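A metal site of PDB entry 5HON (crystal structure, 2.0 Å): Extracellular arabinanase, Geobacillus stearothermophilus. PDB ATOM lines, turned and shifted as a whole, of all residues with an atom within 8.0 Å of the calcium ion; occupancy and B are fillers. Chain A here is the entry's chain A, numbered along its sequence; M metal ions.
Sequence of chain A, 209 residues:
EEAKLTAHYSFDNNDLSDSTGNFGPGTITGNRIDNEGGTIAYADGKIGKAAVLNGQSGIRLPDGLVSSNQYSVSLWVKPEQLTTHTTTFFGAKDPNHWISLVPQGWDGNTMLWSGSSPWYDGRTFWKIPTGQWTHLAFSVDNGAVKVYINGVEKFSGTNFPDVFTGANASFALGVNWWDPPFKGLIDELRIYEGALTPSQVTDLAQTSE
The calcium ion is bound by the backbone carbonyl oxygen (O) of Ser 10 (2.2 Å). OE2 of Glu 188 is bound to the calcium ion. OD1 of Asp 187 binds the calcium ion (2.3 Å). The calcium ion is bound by OD1 of Asp 12. O of Ile 47 is bound to the calcium ion, 2.4 Å away. The calcium ion is bound by O of Lys 49, 2.5 Å away. The calcium ion has six donor atoms within binding distance.
The side-chain carboxylate (OD2) of Asp 187 is in hydrogen-bond range of the backbone NH (N) of Lys 46, 3.0 Å away. The side-chain carboxylate (OE1) of Glu 188 lies within hydrogen-bond range of a ring nitrogen (NE2) of His 8 (2.9 Å). The side-chain amino group (NZ) of Lys 49 is in salt-bridge range of the side-chain carboxylate (OD1) of Asp 44, 2.5 Å away.
Along chain A the residues within 4 Å of the calcium ion span positions 10 to 188. The nearest printed residue that does not touch the calcium ion is Gly 48 (4.1 Å).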
ATOM      1  N   HIS A   8      40.513 -25.918  11.243  1.00  0.00           N
ATOM      2  CA  HIS A   8      39.065 -26.021  11.140  1.00  0.00           C
ATOM      3  C   HIS A   8      38.402 -24.888  11.911  1.00  0.00           C
ATOM      4  O   HIS A   8      38.206 -24.994  13.118  1.00  0.00           O
ATOM      5  CB  HIS A   8      38.578 -27.365  11.677  1.00  0.00           C
ATOM      6  CG  HIS A   8      37.121 -27.611  11.471  1.00  0.00           C
ATOM      7  ND1 HIS A   8      36.392 -28.479  12.263  1.00  0.00           N
ATOM      8  CD2 HIS A   8      36.259 -27.107  10.570  1.00  0.00           C
ATOM      9  CE1 HIS A   8      35.137 -28.495  11.839  1.00  0.00           C
ATOM     10  NE2 HIS A   8      35.028 -27.671  10.820  1.00  0.00           N
ATOM     11  N   TYR A   9      38.094 -23.802  11.233  1.00  0.00           N
ATOM     12  CA  TYR A   9      37.333 -22.741  11.862  1.00  0.00           C
ATOM     13  C   TYR A   9      35.835 -23.017  11.661  1.00  0.00           C
ATOM     14  O   TYR A   9      35.297 -22.816  10.570  1.00  0.00           O
ATOM     15  CB  TYR A   9      37.754 -21.365  11.327  1.00  0.00           C
ATOM     16  CG  TYR A   9      39.170 -21.008  11.706  1.00  0.00           C
ATOM     17  CD1 TYR A   9      39.468 -20.358  12.904  1.00  0.00           C
ATOM     18  CD2 TYR A   9      40.244 -21.355  10.879  1.00  0.00           C
ATOM     19  CE1 TYR A   9      40.783 -20.041  13.251  1.00  0.00           C
ATOM     20  CE2 TYR A   9      41.562 -21.061  11.223  1.00  0.00           C
ATOM     21  CZ  TYR A   9      41.821 -20.394  12.403  1.00  0.00           C
ATOM     22  OH  TYR A   9      43.142 -20.093  12.735  1.00  0.00           O
ATOM     23  N   SER A  10      35.182 -23.479  12.712  1.00  0.00           N
ATOM     24  CA  SER A  10      33.808 -23.974  12.613  1.00  0.00           C
ATOM     25  C   SER A  10      32.771 -23.004  13.179  1.00  0.00           C
ATOM     26  O   SER A  10      31.575 -23.114  12.866  1.00  0.00           O
ATOM     27  CB  SER A  10      33.705 -25.308  13.337  1.00  0.00           C
ATOM     28  OG  SER A  10      33.593 -25.120  14.739  1.00  0.00           O
ATOM     29  N   PHE A  11      33.218 -22.075  14.041  1.00  0.00           N
ATOM     30  CA  PHE A  11      32.351 -21.119  14.742  1.00  0.00           C
ATOM     31  C   PHE A  11      31.314 -21.812  15.635  1.00  0.00           C
ATOM     32  O   PHE A  11      30.501 -21.134  16.269  1.00  0.00           O
ATOM     33  CB  PHE A  11      31.638 -20.194  13.749  1.00  0.00           C
ATOM     34  CG  PHE A  11      32.465 -19.822  12.562  1.00  0.00           C
ATOM     35  CD1 PHE A  11      33.474 -18.888  12.669  1.00  0.00           C
ATOM     36  CD2 PHE A  11      32.249 -20.422  11.323  1.00  0.00           C
ATOM     37  CE1 PHE A  11      34.246 -18.563  11.575  1.00  0.00           C
ATOM     38  CE2 PHE A  11      33.021 -20.106  10.232  1.00  0.00           C
ATOM     39  CZ  PHE A  11      34.015 -19.168  10.354  1.00  0.00           C
ATOM     40  N   ASP A  12      31.349 -23.148  15.687  1.00  0.00           N
ATOM     41  CA  ASP A  12      30.408 -23.956  16.470  1.00  0.00           C
ATOM     42  C   ASP A  12      30.263 -23.499  17.905  1.00  0.00           C
ATOM     43  O   ASP A  12      29.205 -23.632  18.503  1.00  0.00           O
ATOM     44  CB  ASP A  12      30.837 -25.422  16.468  1.00  0.00           C
ATOM     45  CG  ASP A  12      30.434 -26.147  15.225  1.00  0.00           C
ATOM     46  OD1 ASP A  12      30.083 -25.468  14.245  1.00  0.00           O
ATOM     47  OD2 ASP A  12      30.478 -27.405  15.224  1.00  0.00           O
ATOM     48  N   ASN A  13      31.352 -22.988  18.461  1.00  0.00           N
ATOM     49  CA  ASN A  13      31.370 -22.574  19.853  1.00  0.00           C
ATOM     50  C   ASN A  13      31.264 -21.070  19.992  1.00  0.00           C
ATOM     51  O   ASN A  13      31.668 -20.514  21.000  1.00  0.00           O
ATOM     52  CB  ASN A  13      32.649 -23.072  20.517  1.00  0.00           C
ATOM     53  CG  ASN A  13      32.675 -24.583  20.647  1.00  0.00           C
ATOM     54  OD1 ASN A  13      33.434 -25.267  19.954  1.00  0.00           O
ATOM     55  ND2 ASN A  13      31.854 -25.110  21.542  1.00  0.00           N
ATOM     56  N   ASN A  14      30.707 -20.422  18.975  1.00  0.00           N
ATOM     57  CA  ASN A  14      30.471 -18.979  18.970  1.00  0.00           C
ATOM     58  C   ASN A  14      31.746 -18.215  19.320  1.00  0.00           C
ATOM     59  O   ASN A  14      31.737 -17.249  20.089  1.00  0.00           O
ATOM     60  CB  ASN A  14      29.333 -18.632  19.941  1.00  0.00           C
ATOM     61  CG  ASN A  14      28.071 -19.429  19.659  1.00  0.00           C
ATOM     62  OD1 ASN A  14      27.678 -19.620  18.508  1.00  0.00           O
ATOM     63  ND2 ASN A  14      27.447 -19.927  20.729  1.00  0.00           N
ATOM     64  N   TYR A  42      26.709 -14.659  15.726  1.00  0.00           N
ATOM     65  CA  TYR A  42      26.575 -16.086  15.422  1.00  0.00           C
ATOM     66  C   TYR A  42      25.122 -16.537  15.296  1.00  0.00           C
ATOM     67  O   TYR A  42      24.311 -16.384  16.209  1.00  0.00           O
ATOM     68  CB  TYR A  42      27.303 -16.919  16.480  1.00  0.00           C
ATOM     69  CG  TYR A  42      28.795 -16.626  16.522  1.00  0.00           C
ATOM     70  CD1 TYR A  42      29.657 -17.181  15.587  1.00  0.00           C
ATOM     71  CD2 TYR A  42      29.323 -15.772  17.486  1.00  0.00           C
ATOM     72  CE1 TYR A  42      31.028 -16.903  15.615  1.00  0.00           C
ATOM     73  CE2 TYR A  42      30.682 -15.492  17.521  1.00  0.00           C
ATOM     74  CZ  TYR A  42      31.525 -16.058  16.582  1.00  0.00           C
ATOM     75  OH  TYR A  42      32.869 -15.773  16.632  1.00  0.00           O
ATOM     76  N   ALA A  43      24.807 -17.104  14.135  1.00  0.00           N
ATOM     77  CA  ALA A  43      23.476 -17.589  13.819  1.00  0.00           C
ATOM     78  C   ALA A  43      23.553 -19.053  13.419  1.00  0.00           C
ATOM     79  O   ALA A  43      24.643 -19.576  13.147  1.00  0.00           O
ATOM     80  CB  ALA A  43      22.861 -16.772  12.703  1.00  0.00           C
ATOM     81  N   ASP A  44      22.403 -19.706  13.351  1.00  0.00           N
ATOM     82  CA  ASP A  44      22.318 -21.078  12.872  1.00  0.00           C
ATOM     83  C   ASP A  44      22.898 -21.215  11.466  1.00  0.00           C
ATOM     84  O   ASP A  44      22.473 -20.498  10.549  1.00  0.00           O
ATOM     85  CB  ASP A  44      20.874 -21.559  12.899  1.00  0.00           C
ATOM     86  CG  ASP A  44      20.362 -21.743  14.309  1.00  0.00           C
ATOM     87  OD1 ASP A  44      21.083 -21.362  15.252  1.00  0.00           O
ATOM     88  OD2 ASP A  44      19.236 -22.268  14.474  1.00  0.00           O
ATOM     89  N   GLY A  45      23.852 -22.114  11.300  1.00  0.00           N
ATOM     90  CA  GLY A  45      24.533 -22.287  10.024  1.00  0.00           C
ATOM     91  C   GLY A  45      24.372 -23.676   9.450  1.00  0.00           C
ATOM     92  O   GLY A  45      23.564 -24.467   9.923  1.00  0.00           O
ATOM     93  N   LYS A  46      25.158 -23.968   8.415  1.00  0.00           N
ATOM     94  CA  LYS A  46      25.101 -25.258   7.749  1.00  0.00           C
ATOM     95  C   LYS A  46      25.417 -26.403   8.697  1.00  0.00           C
ATOM     96  O   LYS A  46      24.793 -27.461   8.630  1.00  0.00           O
ATOM     97  CB  LYS A  46      26.059 -25.293   6.556  1.00  0.00           C
ATOM     98  CG  LYS A  46      25.974 -26.564   5.734  1.00  0.00           C
ATOM     99  CD  LYS A  46      24.556 -26.774   5.214  1.00  0.00           C
ATOM    100  CE  LYS A  46      24.466 -27.963   4.279  1.00  0.00           C
ATOM    101  NZ  LYS A  46      24.936 -29.217   4.917  1.00  0.00           N
ATOM    102  N   ILE A  47      26.405 -26.198   9.569  1.00  0.00           N
ATOM    103  CA  ILE A  47      26.736 -27.148  10.619  1.00  0.00           C
ATOM    104  C   ILE A  47      26.910 -26.376  11.916  1.00  0.00           C
ATOM    105  O   ILE A  47      27.840 -25.580  12.047  1.00  0.00           O
ATOM    106  CB  ILE A  47      28.030 -27.943  10.305  1.00  0.00           C
ATOM    107  CG1 ILE A  47      27.969 -28.558   8.902  1.00  0.00           C
ATOM    108  CG2 ILE A  47      28.253 -29.025  11.369  1.00  0.00           C
ATOM    109  CD1 ILE A  47      29.244 -29.258   8.480  1.00  0.00           C
ATOM    110  N   GLY A  48      26.013 -26.604  12.876  1.00  0.00           N
ATOM    111  CA  GLY A  48      26.050 -25.879  14.120  1.00  0.00           C
ATOM    112  C   GLY A  48      25.920 -24.396  13.888  1.00  0.00           C
ATOM    113  O   GLY A  48      25.150 -23.958  13.047  1.00  0.00           O
ATOM    114  N   LYS A  49      26.703 -23.618  14.618  1.00  0.00           N
ATOM    115  CA  LYS A  49      26.635 -22.174  14.505  1.00  0.00           C
ATOM    116  C   LYS A  49      27.618 -21.659  13.458  1.00  0.00           C
ATOM    117  O   LYS A  49      28.759 -22.089  13.406  1.00  0.00           O
ATOM    118  CB  LYS A  49      26.907 -21.532  15.859  1.00  0.00           C
ATOM    119  CG  LYS A  49      25.729 -21.618  16.808  1.00  0.00           C
ATOM    120  CD  LYS A  49      24.576 -20.776  16.294  1.00  0.00           C
ATOM    121  CE  LYS A  49      23.421 -20.778  17.281  1.00  0.00           C
ATOM    122  NZ  LYS A  49      22.345 -19.835  16.829  1.00  0.00           N
ATOM    123  N   ALA A  50      27.142 -20.752  12.623  1.00  0.00           N
ATOM    124  CA  ALA A  50      27.970 -20.135  11.607  1.00  0.00           C
ATOM    125  C   ALA A  50      28.266 -18.705  11.996  1.00  0.00           C
ATOM    126  O   ALA A  50      27.586 -18.143  12.847  1.00  0.00           O
ATOM    127  CB  ALA A  50      27.290 -20.203  10.263  1.00  0.00           C
ATOM    128  N   ALA A  51      29.289 -18.118  11.389  1.00  0.00           N
ATOM    129  CA  ALA A  51      29.651 -16.719  11.634  1.00  0.00           C
ATOM    130  C   ALA A  51      28.756 -15.745  10.851  1.00  0.00           C
ATOM    131  O   ALA A  51      28.455 -15.980   9.687  1.00  0.00           O
ATOM    132  CB  ALA A  51      31.120 -16.485  11.282  1.00  0.00           C
ATOM    133  N   TRP A 133      22.755 -21.904   0.827  1.00  0.00           N
ATOM    134  CA  TRP A 133      24.074 -22.434   1.154  1.00  0.00           C
ATOM    135  C   TRP A 133      24.754 -23.039  -0.066  1.00  0.00           C
ATOM    136  O   TRP A 133      24.212 -23.934  -0.696  1.00  0.00           O
ATOM    137  CB  TRP A 133      23.985 -23.508   2.245  1.00  0.00           C
ATOM    138  CG  TRP A 133      23.776 -22.963   3.624  1.00  0.00           C
ATOM    139  CD1 TRP A 133      22.658 -23.081   4.383  1.00  0.00           C
ATOM    140  CD2 TRP A 133      24.706 -22.195   4.393  1.00  0.00           C
ATOM    141  NE1 TRP A 133      22.839 -22.459   5.594  1.00  0.00           N
ATOM    142  CE2 TRP A 133      24.082 -21.900   5.621  1.00  0.00           C
ATOM    143  CE3 TRP A 133      26.010 -21.746   4.178  1.00  0.00           C
ATOM    144  CZ2 TRP A 133      24.712 -21.168   6.631  1.00  0.00           C
ATOM    145  CZ3 TRP A 133      26.630 -21.005   5.182  1.00  0.00           C
ATOM    146  CH2 TRP A 133      25.984 -20.727   6.385  1.00  0.00           C
ATOM    147  N   ILE A 186      29.169 -17.302   6.809  1.00  0.00           N
ATOM    148  CA  ILE A 186      30.281 -18.180   6.460  1.00  0.00           C
ATOM    149  C   ILE A 186      30.441 -19.271   7.527  1.00  0.00           C
ATOM    150  O   ILE A 186      30.487 -18.966   8.718  1.00  0.00           O
ATOM    151  CB  ILE A 186      31.607 -17.398   6.320  1.00  0.00           C
ATOM    152  CG1 ILE A 186      31.554 -16.461   5.113  1.00  0.00           C
ATOM    153  CG2 ILE A 186      32.776 -18.360   6.187  1.00  0.00           C
ATOM    154  CD1 ILE A 186      32.908 -15.825   4.752  1.00  0.00           C
ATOM    155  N   ASP A 187      30.515 -20.531   7.112  1.00  0.00           N
ATOM    156  CA  ASP A 187      30.575 -21.644   8.066  1.00  0.00           C
ATOM    157  C   ASP A 187      31.683 -22.632   7.692  1.00  0.00           C
ATOM    158  O   ASP A 187      32.055 -22.756   6.520  1.00  0.00           O
ATOM    159  CB  ASP A 187      29.225 -22.365   8.127  1.00  0.00           C
ATOM    160  CG  ASP A 187      29.006 -23.093   9.448  1.00  0.00           C
ATOM    161  OD1 ASP A 187      29.974 -23.242  10.206  1.00  0.00           O
ATOM    162  OD2 ASP A 187      27.867 -23.522   9.733  1.00  0.00           O
ATOM    163  N   GLU A 188      32.207 -23.337   8.693  1.00  0.00           N
ATOM    164  CA  GLU A 188      33.054 -24.501   8.469  1.00  0.00           C
ATOM    165  C   GLU A 188      34.272 -24.252   7.585  1.00  0.00           C
ATOM    166  O   GLU A 188      34.420 -24.851   6.529  1.00  0.00           O
ATOM    167  CB  GLU A 188      32.212 -25.620   7.858  1.00  0.00           C
ATOM    168  CG  GLU A 188      30.976 -25.900   8.669  1.00  0.00           C
ATOM    169  CD  GLU A 188      31.321 -26.254  10.100  1.00  0.00           C
ATOM    170  OE1 GLU A 188      32.250 -27.050  10.299  1.00  0.00           O
ATOM    171  OE2 GLU A 188      30.689 -25.709  11.037  1.00  0.00           O
ATOM    172  N   LEU A 189      35.155 -23.350   8.019  1.00  0.00           N
ATOM    173  CA  LEU A 189      36.369 -23.117   7.258  1.00  0.00           C
ATOM    174  C   LEU A 189      37.353 -24.214   7.604  1.00  0.00           C
ATOM    175  O   LEU A 189      37.611 -24.476   8.774  1.00  0.00           O
ATOM    176  CB  LEU A 189      36.960 -21.726   7.547  1.00  0.00           C
ATOM    177  CG  LEU A 189      38.345 -21.451   6.938  1.00  0.00           C
ATOM    178  CD1 LEU A 189      38.378 -21.806   5.460  1.00  0.00           C
ATOM    179  CD2 LEU A 189      38.745 -19.990   7.145  1.00  0.00           C
HETATM  180 CA    CA M   1      29.709 -24.160  12.328  1.00  0.00          CA
